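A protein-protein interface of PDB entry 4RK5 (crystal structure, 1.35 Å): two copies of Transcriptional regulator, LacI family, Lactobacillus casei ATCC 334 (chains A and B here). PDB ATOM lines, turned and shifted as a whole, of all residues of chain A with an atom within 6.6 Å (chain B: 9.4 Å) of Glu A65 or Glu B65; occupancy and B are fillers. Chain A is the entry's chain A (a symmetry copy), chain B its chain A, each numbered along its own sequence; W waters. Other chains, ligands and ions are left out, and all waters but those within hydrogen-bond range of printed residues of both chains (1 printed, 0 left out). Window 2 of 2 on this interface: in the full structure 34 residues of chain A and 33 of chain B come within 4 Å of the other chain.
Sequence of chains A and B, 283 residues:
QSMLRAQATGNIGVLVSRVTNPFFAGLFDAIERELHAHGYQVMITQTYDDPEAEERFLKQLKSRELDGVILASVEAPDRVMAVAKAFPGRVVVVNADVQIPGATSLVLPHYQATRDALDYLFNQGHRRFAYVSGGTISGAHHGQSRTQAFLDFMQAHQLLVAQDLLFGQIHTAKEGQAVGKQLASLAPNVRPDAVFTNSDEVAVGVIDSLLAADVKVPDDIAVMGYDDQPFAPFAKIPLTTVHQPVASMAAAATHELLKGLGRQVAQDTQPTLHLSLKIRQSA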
ATOM      1  N   GLY A  10      16.011  20.223 -27.541  1.00  0.00           N
ATOM      2  CA  GLY A  10      14.991  20.349 -26.514  1.00  0.00           C
ATOM      3  C   GLY A  10      15.433  19.967 -25.072  1.00  0.00           C
ATOM      4  O   GLY A  10      16.478  20.414 -24.637  1.00  0.00           O
ATOM      5  N   ASN A  11      14.575  19.145 -24.433  1.00  0.00           N
ATOM      6  CA  ASN A  11      14.772  18.774 -23.026  1.00  0.00           C
ATOM      7  C   ASN A  11      15.206  17.329 -22.904  1.00  0.00           C
ATOM      8  O   ASN A  11      14.604  16.463 -23.547  1.00  0.00           O
ATOM      9  CB  ASN A  11      13.486  18.967 -22.215  1.00  0.00           C
ATOM     10  CG  ASN A  11      13.071  20.420 -22.147  1.00  0.00           C
ATOM     11  OD1 ASN A  11      13.880  21.321 -22.129  1.00  0.00           O
ATOM     12  ND2 ASN A  11      11.776  20.644 -22.052  1.00  0.00           N
ATOM     13  N   ILE A  12      16.258  17.088 -22.097  1.00  0.00           N
ATOM     14  CA  ILE A  12      16.727  15.734 -21.839  1.00  0.00           C
ATOM     15  C   ILE A  12      16.631  15.508 -20.349  1.00  0.00           C
ATOM     16  O   ILE A  12      16.981  16.389 -19.532  1.00  0.00           O
ATOM     17  CB  ILE A  12      18.181  15.554 -22.288  1.00  0.00           C
ATOM     18  CG1 ILE A  12      18.372  15.900 -23.789  1.00  0.00           C
ATOM     19  CG2 ILE A  12      18.720  14.192 -21.926  1.00  0.00           C
ATOM     20  CD1 ILE A  12      17.565  15.055 -24.657  1.00  0.00           C
ATOM     21  N   MET A  43      17.761  18.045 -17.197  1.00  0.00           N
ATOM     22  CA  MET A  43      17.237  18.029 -15.835  1.00  0.00           C
ATOM     23  C   MET A  43      17.452  16.648 -15.257  1.00  0.00           C
ATOM     24  O   MET A  43      17.343  15.650 -15.978  1.00  0.00           O
ATOM     25  CB  MET A  43      15.731  18.353 -15.911  1.00  0.00           C
ATOM     26  CG  MET A  43      15.582  19.779 -16.710  1.00  0.00           C
ATOM     27  SD  MET A  43      14.922  19.343 -18.498  1.00  0.00           S
ATOM     28  CE  MET A  43      13.247  18.993 -17.405  1.00  0.00           C
ATOM     29  N   LYS A  59       7.246   8.563 -17.908  1.00  0.00           N
ATOM     30  CA  LYS A  59       6.029   9.171 -18.470  1.00  0.00           C
ATOM     31  C   LYS A  59       6.321  10.494 -19.121  1.00  0.00           C
ATOM     32  O   LYS A  59       5.601  10.903 -20.046  1.00  0.00           O
ATOM     33  CB  LYS A  59       4.901   9.339 -17.425  1.00  0.00           C
ATOM     34  CG  LYS A  59       4.258   8.051 -16.974  1.00  0.00           C
ATOM     35  CD  LYS A  59       3.148   8.281 -15.942  1.00  0.00           C
ATOM     36  CE  LYS A  59       2.696   6.929 -15.402  1.00  0.00           C
ATOM     37  NZ  LYS A  59       1.696   7.099 -14.349  1.00  0.00           N
ATOM     38  N   GLN A  60       7.358  11.173 -18.664  1.00  0.00           N
ATOM     39  CA  GLN A  60       7.741  12.412 -19.320  1.00  0.00           C
ATOM     40  C   GLN A  60       8.211  12.272 -20.779  1.00  0.00           C
ATOM     41  O   GLN A  60       8.050  13.157 -21.669  1.00  0.00           O
ATOM     42  CB  GLN A  60       8.827  13.087 -18.491  1.00  0.00           C
ATOM     43  CG  GLN A  60       8.380  13.504 -17.093  1.00  0.00           C
ATOM     44  CD  GLN A  60       8.407  15.010 -16.955  1.00  0.00           C
ATOM     45  OE1 GLN A  60       9.397  15.592 -16.476  1.00  0.00           O
ATOM     46  NE2 GLN A  60       7.333  15.662 -17.369  1.00  0.00           N
ATOM     47  N   LEU A  61       8.878  11.125 -20.987  1.00  0.00           N
ATOM     48  CA  LEU A  61       9.280  10.811 -22.348  1.00  0.00           C
ATOM     49  C   LEU A  61       8.047  10.345 -23.138  1.00  0.00           C
ATOM     50  O   LEU A  61       7.836  10.775 -24.268  1.00  0.00           O
ATOM     51  CB  LEU A  61      10.375   9.704 -22.331  1.00  0.00           C
ATOM     52  CG  LEU A  61      10.895   9.332 -23.697  1.00  0.00           C
ATOM     53  CD1 LEU A  61      11.615  10.484 -24.260  1.00  0.00           C
ATOM     54  CD2 LEU A  61      11.727   8.070 -23.608  1.00  0.00           C
ATOM     55  N   LYS A  62       7.208   9.517 -22.484  1.00  0.00           N
ATOM     56  CA  LYS A  62       6.004   8.980 -23.176  1.00  0.00           C
ATOM     57  C   LYS A  62       5.036  10.069 -23.646  1.00  0.00           C
ATOM     58  O   LYS A  62       4.419   9.916 -24.688  1.00  0.00           O
ATOM     59  CB  LYS A  62       5.269   7.883 -22.388  1.00  0.00           C
ATOM     60  CG  LYS A  62       6.123   6.655 -22.243  1.00  0.00           C
ATOM     61  CD  LYS A  62       5.367   5.408 -21.858  1.00  0.00           C
ATOM     62  CE  LYS A  62       4.879   5.541 -20.492  1.00  0.00           C
ATOM     63  NZ  LYS A  62       4.015   4.406 -20.183  1.00  0.00           N
ATOM     64  N   SER A  63       4.976  11.176 -22.843  1.00  0.00           N
ATOM     65  CA  SER A  63       4.151  12.324 -23.166  1.00  0.00           C
ATOM     66  C   SER A  63       4.896  13.406 -24.009  1.00  0.00           C
ATOM     67  O   SER A  63       4.315  14.454 -24.335  1.00  0.00           O
ATOM     68  CB  SER A  63       3.514  12.878 -21.897  1.00  0.00           C
ATOM     69  OG  SER A  63       2.757  11.840 -21.195  1.00  0.00           O
ATOM     70  N   ARG A  64       6.146  13.103 -24.388  1.00  0.00           N
ATOM     71  CA  ARG A  64       6.982  13.994 -25.230  1.00  0.00           C
ATOM     72  C   ARG A  64       7.290  15.374 -24.624  1.00  0.00           C
ATOM     73  O   ARG A  64       7.678  16.312 -25.291  1.00  0.00           O
ATOM     74  CB  ARG A  64       6.489  14.007 -26.665  1.00  0.00           C
ATOM     75  CG  ARG A  64       6.765  12.625 -27.320  1.00  0.00           C
ATOM     76  CD  ARG A  64       8.251  12.110 -27.166  1.00  0.00           C
ATOM     77  NE  ARG A  64       9.216  13.166 -27.522  1.00  0.00           N
ATOM     78  CZ  ARG A  64       9.440  13.561 -28.769  1.00  0.00           C
ATOM     79  NH1 ARG A  64       8.824  12.944 -29.814  1.00  0.00           N
ATOM     80  NH2 ARG A  64      10.282  14.600 -28.997  1.00  0.00           N
ATOM     81  N   GLU A  65       7.217  15.444 -23.302  1.00  0.00           N
ATOM     82  CA  GLU A  65       7.823  16.521 -22.514  1.00  0.00           C
ATOM     83  C   GLU A  65       9.368  16.524 -22.634  1.00  0.00           C
ATOM     84  O   GLU A  65      10.000  17.560 -22.577  1.00  0.00           O
ATOM     85  CB  GLU A  65       7.343  16.497 -21.054  1.00  0.00           C
ATOM     86  CG  GLU A  65       6.397  17.642 -20.698  1.00  0.00           C
ATOM     87  CD  GLU A  65       5.546  17.391 -19.457  1.00  0.00           C
ATOM     88  OE1 GLU A  65       5.683  18.142 -18.456  1.00  0.00           O
ATOM     89  OE2 GLU A  65       4.728  16.446 -19.488  1.00  0.00           O
ATOM     90  N   LEU A  66       9.946  15.334 -22.741  1.00  0.00           N
ATOM     91  CA  LEU A  66      11.335  15.156 -22.990  1.00  0.00           C
ATOM     92  C   LEU A  66      11.600  14.598 -24.373  1.00  0.00           C
ATOM     93  O   LEU A  66      10.795  13.790 -24.816  1.00  0.00           O
ATOM     94  CB  LEU A  66      11.940  14.199 -21.964  1.00  0.00           C
ATOM     95  CG  LEU A  66      11.841  14.617 -20.498  1.00  0.00           C
ATOM     96  CD1 LEU A  66      12.295  13.499 -19.595  1.00  0.00           C
ATOM     97  CD2 LEU A  66      12.586  15.917 -20.213  1.00  0.00           C
ATOM     98  N   ASP A  67      12.665  15.037 -25.022  1.00  0.00           N
ATOM     99  CA  ASP A  67      13.217  14.419 -26.224  1.00  0.00           C
ATOM    100  C   ASP A  67      13.878  13.063 -26.007  1.00  0.00           C
ATOM    101  O   ASP A  67      13.880  12.231 -26.893  1.00  0.00           O
ATOM    102  CB  ASP A  67      14.188  15.351 -26.937  1.00  0.00           C
ATOM    103  CG  ASP A  67      13.507  16.538 -27.564  1.00  0.00           C
ATOM    104  OD1 ASP A  67      12.276  16.654 -27.469  1.00  0.00           O
ATOM    105  OD2 ASP A  67      14.229  17.355 -28.135  1.00  0.00           O
ATOM    106  N   GLY B  10       1.950  17.691  -9.324  1.00  0.00           N
ATOM    107  CA  GLY B  10       2.631  17.617 -10.605  1.00  0.00           C
ATOM    108  C   GLY B  10       4.184  17.692 -10.550  1.00  0.00           C
ATOM    109  O   GLY B  10       4.781  16.991  -9.753  1.00  0.00           O
ATOM    110  N   ASN B  11       4.725  18.562 -11.427  1.00  0.00           N
ATOM    111  CA  ASN B  11       6.179  18.678 -11.595  1.00  0.00           C
ATOM    112  C   ASN B  11       6.689  19.978 -11.009  1.00  0.00           C
ATOM    113  O   ASN B  11       6.092  21.028 -11.266  1.00  0.00           O
ATOM    114  CB  ASN B  11       6.574  18.623 -13.074  1.00  0.00           C
ATOM    115  CG  ASN B  11       6.248  17.284 -13.700  1.00  0.00           C
ATOM    116  OD1 ASN B  11       6.300  16.250 -13.071  1.00  0.00           O
ATOM    117  ND2 ASN B  11       5.957  17.305 -14.983  1.00  0.00           N
ATOM    118  N   ILE B  12       7.772  19.890 -10.213  1.00  0.00           N
ATOM    119  CA  ILE B  12       8.401  21.074  -9.647  1.00  0.00           C
ATOM    120  C   ILE B  12       9.830  21.095 -10.137  1.00  0.00           C
ATOM    121  O   ILE B  12      10.522  20.052 -10.171  1.00  0.00           O
ATOM    122  CB  ILE B  12       8.390  21.031  -8.115  1.00  0.00           C
ATOM    123  CG1 ILE B  12       6.954  20.878  -7.549  1.00  0.00           C
ATOM    124  CG2 ILE B  12       9.138  22.194  -7.512  1.00  0.00           C
ATOM    125  CD1 ILE B  12       6.087  21.981  -7.937  1.00  0.00           C
ATOM    126  N   GLY B  13      10.326  22.288 -10.494  1.00  0.00           N
ATOM    127  CA  GLY B  13      11.733  22.458 -10.864  1.00  0.00           C
ATOM    128  C   GLY B  13      12.512  23.167  -9.779  1.00  0.00           C
ATOM    129  O   GLY B  13      11.976  24.049  -9.090  1.00  0.00           O
ATOM    130  N   TYR B  40       4.712  15.167  -5.511  1.00  0.00           N
ATOM    131  CA  TYR B  40       5.332  15.825  -6.641  1.00  0.00           C
ATOM    132  C   TYR B  40       6.552  15.108  -7.161  1.00  0.00           C
ATOM    133  O   TYR B  40       7.236  14.399  -6.426  1.00  0.00           O
ATOM    134  CB  TYR B  40       5.736  17.258  -6.228  1.00  0.00           C
ATOM    135  CG  TYR B  40       4.588  18.164  -5.971  1.00  0.00           C
ATOM    136  CD1 TYR B  40       4.041  18.871  -7.021  1.00  0.00           C
ATOM    137  CD2 TYR B  40       4.035  18.261  -4.691  1.00  0.00           C
ATOM    138  CE1 TYR B  40       2.946  19.708  -6.825  1.00  0.00           C
ATOM    139  CE2 TYR B  40       2.904  19.053  -4.484  1.00  0.00           C
ATOM    140  CZ  TYR B  40       2.385  19.796  -5.559  1.00  0.00           C
ATOM    141  OH  TYR B  40       1.287  20.596  -5.370  1.00  0.00           O
ATOM    142  N   GLN B  41       6.791  15.313  -8.463  1.00  0.00           N
ATOM    143  CA  GLN B  41       8.027  14.892  -9.124  1.00  0.00           C
ATOM    144  C   GLN B  41       8.907  16.150  -9.246  1.00  0.00           C
ATOM    145  O   GLN B  41       8.447  17.166  -9.682  1.00  0.00           O
ATOM    146  CB  GLN B  41       7.737  14.350 -10.498  1.00  0.00           C
ATOM    147  CG  GLN B  41       8.951  13.988 -11.315  1.00  0.00           C
ATOM    148  CD  GLN B  41       8.549  13.171 -12.513  1.00  0.00           C
ATOM    149  OE1 GLN B  41       9.032  12.108 -12.694  1.00  0.00           O
ATOM    150  NE2 GLN B  41       7.663  13.719 -13.374  1.00  0.00           N
ATOM    151  N   MET B  43      12.611  17.953 -10.354  1.00  0.00           N
ATOM    152  CA  MET B  43      13.767  17.872 -11.242  1.00  0.00           C
ATOM    153  C   MET B  43      14.638  19.086 -11.005  1.00  0.00           C
ATOM    154  O   MET B  43      14.122  20.180 -10.753  1.00  0.00           O
ATOM    155  CB  MET B  43      13.240  17.863 -12.691  1.00  0.00           C
ATOM    156  CG  MET B  43      12.168  16.624 -12.809  1.00  0.00           C
ATOM    157  SD  MET B  43      10.390  17.437 -12.850  1.00  0.00           S
ATOM    158  CE  MET B  43      11.056  17.943 -14.701  1.00  0.00           C
ATOM    159  N   ARG B  56      15.731  29.965 -19.790  1.00  0.00           N
ATOM    160  CA  ARG B  56      15.195  28.755 -20.416  1.00  0.00           C
ATOM    161  C   ARG B  56      14.418  27.909 -19.410  1.00  0.00           C
ATOM    162  O   ARG B  56      13.344  27.360 -19.719  1.00  0.00           O
ATOM    163  CB  ARG B  56      16.318  28.035 -21.055  1.00  0.00           C
ATOM    164  CG  ARG B  56      15.801  26.969 -21.967  1.00  0.00           C
ATOM    165  CD  ARG B  56      16.893  26.397 -22.783  1.00  0.00           C
ATOM    166  NE  ARG B  56      16.377  25.341 -23.644  1.00  0.00           N
ATOM    167  CZ  ARG B  56      17.179  24.620 -24.427  1.00  0.00           C
ATOM    168  NH1 ARG B  56      18.474  24.886 -24.410  1.00  0.00           N
ATOM    169  NH2 ARG B  56      16.660  23.660 -25.169  1.00  0.00           N
ATOM    170  N   PHE B  57      14.962  27.767 -18.196  1.00  0.00           N
ATOM    171  CA  PHE B  57      14.313  27.012 -17.139  1.00  0.00           C
ATOM    172  C   PHE B  57      12.923  27.615 -16.818  1.00  0.00           C
ATOM    173  O   PHE B  57      11.930  26.895 -16.709  1.00  0.00           O
ATOM    174  CB  PHE B  57      15.238  26.969 -15.906  1.00  0.00           C
ATOM    175  CG  PHE B  57      14.574  26.517 -14.595  1.00  0.00           C
ATOM    176  CD1 PHE B  57      14.536  25.256 -14.276  1.00  0.00           C
ATOM    177  CD2 PHE B  57      14.001  27.446 -13.681  1.00  0.00           C
ATOM    178  CE1 PHE B  57      13.974  24.786 -13.089  1.00  0.00           C
ATOM    179  CE2 PHE B  57      13.440  27.041 -12.514  1.00  0.00           C
ATOM    180  CZ  PHE B  57      13.446  25.686 -12.181  1.00  0.00           C
ATOM    181  N   LEU B  58      12.892  28.946 -16.697  1.00  0.00           N
ATOM    182  CA  LEU B  58      11.658  29.645 -16.376  1.00  0.00           C
ATOM    183  C   LEU B  58      10.605  29.493 -17.472  1.00  0.00           C
ATOM    184  O   LEU B  58       9.422  29.527 -17.153  1.00  0.00           O
ATOM    185  CB  LEU B  58      11.936  31.111 -16.046  1.00  0.00           C
ATOM    186  CG  LEU B  58      12.666  31.281 -14.731  1.00  0.00           C
ATOM    187  CD1 LEU B  58      13.032  32.749 -14.645  1.00  0.00           C
ATOM    188  CD2 LEU B  58      11.940  30.812 -13.515  1.00  0.00           C
ATOM    189  N   LYS B  59      11.046  29.300 -18.708  1.00  0.00           N
ATOM    190  CA  LYS B  59      10.080  29.028 -19.785  1.00  0.00           C
ATOM    191  C   LYS B  59       9.283  27.783 -19.513  1.00  0.00           C
ATOM    192  O   LYS B  59       8.141  27.662 -19.985  1.00  0.00           O
ATOM    193  CB  LYS B  59      10.742  28.932 -21.179  1.00  0.00           C
ATOM    194  CG  LYS B  59      11.251  30.241 -21.731  1.00  0.00           C
ATOM    195  CD  LYS B  59      11.894  30.084 -23.113  1.00  0.00           C
ATOM    196  CE  LYS B  59      12.550  31.403 -23.500  1.00  0.00           C
ATOM    197  NZ  LYS B  59      13.252  31.279 -24.777  1.00  0.00           N
ATOM    198  N   GLN B  60       9.852  26.857 -18.764  1.00  0.00           N
ATOM    199  CA  GLN B  60       9.091  25.676 -18.392  1.00  0.00           C
ATOM    200  C   GLN B  60       7.861  25.933 -17.503  1.00  0.00           C
ATOM    201  O   GLN B  60       6.805  25.236 -17.527  1.00  0.00           O
ATOM    202  CB  GLN B  60      10.026  24.689 -17.704  1.00  0.00           C
ATOM    203  CG  GLN B  60      11.152  24.167 -18.593  1.00  0.00           C
ATOM    204  CD  GLN B  60      10.996  22.681 -18.827  1.00  0.00           C
ATOM    205  OE1 GLN B  60      11.594  21.854 -18.116  1.00  0.00           O
ATOM    206  NE2 GLN B  60      10.198  22.318 -19.818  1.00  0.00           N
ATOM    207  N   LEU B  61       8.061  26.947 -16.645  1.00  0.00           N
ATOM    208  CA  LEU B  61       6.939  27.371 -15.823  1.00  0.00           C
ATOM    209  C   LEU B  61       5.962  28.179 -16.693  1.00  0.00           C
ATOM    210  O   LEU B  61       4.755  27.967 -16.627  1.00  0.00           O
ATOM    211  CB  LEU B  61       7.456  28.229 -14.631  1.00  0.00           C
ATOM    212  CG  LEU B  61       6.371  28.688 -13.690  1.00  0.00           C
ATOM    213  CD1 LEU B  61       5.802  27.513 -13.013  1.00  0.00           C
ATOM    214  CD2 LEU B  61       6.917  29.738 -12.744  1.00  0.00           C
ATOM    215  N   LYS B  62       6.523  29.049 -17.554  1.00  0.00           N
ATOM    216  CA  LYS B  62       5.659  29.905 -18.414  1.00  0.00           C
ATOM    217  C   LYS B  62       4.751  29.106 -19.353  1.00  0.00           C
ATOM    218  O   LYS B  62       3.635  29.526 -19.611  1.00  0.00           O
ATOM    219  CB  LYS B  62       6.427  30.997 -19.178  1.00  0.00           C
ATOM    220  CG  LYS B  62       7.025  32.001 -18.233  1.00  0.00           C
ATOM    221  CD  LYS B  62       7.435  33.301 -18.879  1.00  0.00           C
ATOM    222  CE  LYS B  62       8.574  33.068 -19.756  1.00  0.00           C
ATOM    223  NZ  LYS B  62       8.862  34.292 -20.497  1.00  0.00           N
ATOM    224  N   SER B  63       5.280  27.926 -19.804  1.00  0.00           N
ATOM    225  CA  SER B  63       4.536  27.021 -20.658  1.00  0.00           C
ATOM    226  C   SER B  63       3.722  25.949 -19.867  1.00  0.00           C
ATOM    227  O   SER B  63       3.059  25.093 -20.475  1.00  0.00           O
ATOM    228  CB  SER B  63       5.464  26.421 -21.709  1.00  0.00           C
ATOM    229  OG  SER B  63       6.132  27.473 -22.478  1.00  0.00           O
ATOM    230  N   ARG B  64       3.749  26.056 -18.530  1.00  0.00           N
ATOM    231  CA  ARG B  64       2.996  25.152 -17.625  1.00  0.00           C
ATOM    232  C   ARG B  64       3.382  23.664 -17.711  1.00  0.00           C
ATOM    233  O   ARG B  64       2.669  22.776 -17.287  1.00  0.00           O
ATOM    234  CB  ARG B  64       1.508  25.444 -17.677  1.00  0.00           C
ATOM    235  CG  ARG B  64       1.230  26.827 -17.024  1.00  0.00           C
ATOM    236  CD  ARG B  64       1.862  27.015 -15.588  1.00  0.00           C
ATOM    237  NE  ARG B  64       1.571  25.855 -14.726  1.00  0.00           N
ATOM    238  CZ  ARG B  64       0.374  25.610 -14.210  1.00  0.00           C
ATOM    239  NH1 ARG B  64      -0.654  26.480 -14.399  1.00  0.00           N
ATOM    240  NH2 ARG B  64       0.175  24.471 -13.499  1.00  0.00           N
ATOM    241  N   GLU B  65       4.599  23.419 -18.173  1.00  0.00           N
ATOM    242  CA  GLU B  65       5.292  22.140 -17.987  1.00  0.00           C
ATOM    243  C   GLU B  65       5.581  21.855 -16.491  1.00  0.00           C
ATOM    244  O   GLU B  65       5.598  20.718 -16.061  1.00  0.00           O
ATOM    245  CB  GLU B  65       6.553  22.045 -18.861  1.00  0.00           C
ATOM    246  CG  GLU B  65       6.420  21.066 -20.026  1.00  0.00           C
ATOM    247  CD  GLU B  65       7.422  21.293 -21.154  1.00  0.00           C
ATOM    248  OE1 GLU B  65       8.258  20.392 -21.425  1.00  0.00           O
ATOM    249  OE2 GLU B  65       7.364  22.373 -21.782  1.00  0.00           O
ATOM    250  N   LEU B  66       5.861  22.913 -15.739  1.00  0.00           N
ATOM    251  CA  LEU B  66       6.022  22.850 -14.328  1.00  0.00           C
ATOM    252  C   LEU B  66       4.892  23.542 -13.594  1.00  0.00           C
ATOM    253  O   LEU B  66       4.420  24.548 -14.109  1.00  0.00           O
ATOM    254  CB  LEU B  66       7.336  23.512 -13.914  1.00  0.00           C
ATOM    255  CG  LEU B  66       8.616  22.912 -14.494  1.00  0.00           C
ATOM    256  CD1 LEU B  66       9.805  23.776 -14.164  1.00  0.00           C
ATOM    257  CD2 LEU B  66       8.826  21.464 -14.062  1.00  0.00           C
ATOM    258  N   ASP B  67       4.469  23.004 -12.463  1.00  0.00           N
ATOM    259  CA  ASP B  67       3.597  23.672 -11.502  1.00  0.00           C
ATOM    260  C   ASP B  67       4.237  24.826 -10.742  1.00  0.00           C
ATOM    261  O   ASP B  67       3.562  25.763 -10.361  1.00  0.00           O
ATOM    262  CB  ASP B  67       2.994  22.683 -10.512  1.00  0.00           C
ATOM    263  CG  ASP B  67       1.993  21.755 -11.147  1.00  0.00           C
ATOM    264  OD1 ASP B  67       1.740  21.869 -12.356  1.00  0.00           O
ATOM    265  OD2 ASP B  67       1.482  20.905 -10.418  1.00  0.00           O
ATOM    266  N   GLY B  68       5.524  24.688 -10.433  1.00  0.00           N
ATOM    267  CA  GLY B  68       6.195  25.643  -9.599  1.00  0.00           C
ATOM    268  C   GLY B  68       7.698  25.437  -9.670  1.00  0.00           C
ATOM    269  O   GLY B  68       8.164  24.408 -10.154  1.00  0.00           O
ATOM    270  N   VAL B  69       8.439  26.446  -9.157  1.00  0.00           N
ATOM    271  CA  VAL B  69       9.886  26.418  -9.167  1.00  0.00           C
ATOM    272  C   VAL B  69      10.445  27.001  -7.866  1.00  0.00           C
ATOM    273  O   VAL B  69       9.872  27.928  -7.267  1.00  0.00           O
ATOM    274  CB  VAL B  69      10.492  27.169 -10.351  1.00  0.00           C
ATOM    275  CG1 VAL B  69      10.083  26.565 -11.704  1.00  0.00           C
ATOM    276  CG2 VAL B  69      10.129  28.630 -10.260  1.00  0.00           C
ATOM    277  N   PHE B  87       2.987  34.518 -12.473  1.00  0.00           N
ATOM    278  CA  PHE B  87       2.689  33.172 -11.924  1.00  0.00           C
ATOM    279  C   PHE B  87       2.697  33.251 -10.409  1.00  0.00           C
ATOM    280  O   PHE B  87       3.543  32.625  -9.715  1.00  0.00           O
ATOM    281  CB  PHE B  87       3.729  32.150 -12.456  1.00  0.00           C
ATOM    282  CG  PHE B  87       3.571  31.915 -13.958  1.00  0.00           C
ATOM    283  CD1 PHE B  87       4.127  32.764 -14.889  1.00  0.00           C
ATOM    284  CD2 PHE B  87       2.754  30.903 -14.413  1.00  0.00           C
ATOM    285  CE1 PHE B  87       3.845  32.595 -16.231  1.00  0.00           C
ATOM    286  CE2 PHE B  87       2.476  30.745 -15.762  1.00  0.00           C
ATOM    287  CZ  PHE B  87       3.045  31.589 -16.671  1.00  0.00           C
ATOM    288  N   ARG B  90       3.837  30.504  -7.469  1.00  0.00           N
ATOM    289  CA  ARG B  90       4.548  29.396  -8.131  1.00  0.00           C
ATOM    290  C   ARG B  90       6.061  29.572  -8.190  1.00  0.00           C
ATOM    291  O   ARG B  90       6.758  28.625  -8.609  1.00  0.00           O
ATOM    292  CB  ARG B  90       4.032  29.219  -9.539  1.00  0.00           C
ATOM    293  CG  ARG B  90       2.538  28.885  -9.621  1.00  0.00           C
ATOM    294  CD  ARG B  90       2.105  28.630 -11.036  1.00  0.00           C
ATOM    295  NE  ARG B  90       0.677  28.455 -11.128  1.00  0.00           N
ATOM    296  CZ  ARG B  90       0.047  27.323 -10.965  1.00  0.00           C
ATOM    297  NH1 ARG B  90       0.717  26.209 -10.684  1.00  0.00           N
ATOM    298  NH2 ARG B  90      -1.287  27.276 -11.053  1.00  0.00           N
HETATM  299  O   HOH W   1      14.028  23.059 -24.177  1.00  0.00           O
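N of Leu A66 lies within hydrogen-bond range of O of Gln A60, at 3.1 Å.
The backbone NH (N) of Ile B12 sits at hydrogen-bond distance from the backbone carbonyl oxygen (O) of Gln B41, 2.9 Å away.
The backbone carbonyl oxygen of Ile A12 lies within hydrogen-bond range of the backbone NH of Met A43, 3.0 Å away.
The backbone carbonyl oxygen (O) of Asn B11 sits at hydrogen-bond distance from the backbone NH (N) of Asp B67.
OD1 of Asn B11 lies within hydrogen-bond range of NE2 of Gln B41.
The backbone carbonyl oxygen (O) of Gln A60 lies within hydrogen-bond range of the backbone NH (N) of Glu A65, 2.9 Å away.
Asn A11 touches Gln B60, and with the chains exchanged Gln A60 touches Asn B11.
Asn A11 touches Glu B65, and with the chains exchanged Glu A65 touches Asn B11.
Met A43 touches Gln B60, and with the chains exchanged Gln A60 touches Met B43.
Glu B65 touches its own counterpart, Glu A65.
Positions printed for both chains: 10, 11, 12, 43, 59, 60, 61, 62, 63, 64, 65, 66 and 67.
Printed residues of chain B within 4 Å of Gln A60: Asn B11 (3.2 Å), Gln B41 (3.8 Å) and Met B43 (3.4 Å).
Glu A65 touches just these residues of chain B: Asn B11 (3.6 Å) and Glu B65 (3.4 Å).
No residue of chain B comes within 4 Å of Leu A66.
Printed residues of chain A within 4 Å of Asn B11: Gln A60 and Glu A65.
Of the printed residues of chain A, Gln B41 touches Gln A60.
Of the printed residues of chain A, Met B43 touches Met A43 and Gln A60.
Of the printed residues of chain A, Arg B56 touches Gly A10.
Lys B59 touches none of the printed residues of chain A.
Glu B65 touches two residues of chain A.
The nearest printed residue of chain A that does not touch Glu B65 is Leu A66 (5.5 Å).
The nearest printed residue of chain A that does not touch Arg B56 is Asn A11 (4.7 Å).
Among the printed residues, merely in contact across the chains: Asn A11 with Glu B65 (3.6 Å), Met A43 with Met B43 (3.6 Å), Met A43 with Gln B60 (3.4 Å), Gln A60 with Gln B41 (3.8 Å), Gln A60 with Met B43 (3.4 Å), Glu A65 with Asn B11 (3.6 Å) and Glu A65 with Glu B65 (3.4 Å).
Water W1 bridges OD1 of Asn A11 and NH2 of Arg B56.
The guanidinium group (NH2) of Arg B56 sits at hydrogen-bond distance from the backbone carbonyl oxygen (O) of Gly A10.
The side-chain amide nitrogen (NE2) of Gln B60 lies close to the side-chain amide nitrogen (ND2) of Asn A11, 3.2 Å away.
The side-chain amide nitrogen (NE2) of Gln A60 sits close to the side-chain amide nitrogen (ND2) of Asn B11.
Of the 13 printed residues of chain A, 5 touch a printed residue of chain B.
Hydrophobic or aromatic side chains of chain A that line the printed part of chain B: Met A43.
Of the 23 printed residues of chain B, 6 touch a printed residue of chain A.
Printed residues of chain B that touch a printed residue of chain A: Asn B11, Gln B41, Met B43, Arg B56, Gln B60 and Glu B65.
Among the printed residues, 10 pairs touch across the chains.
Among the printed residues, no Asp or Glu carboxylate lies within 4 Å of a Lys or Arg side-chain nitrogen of the other chain.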
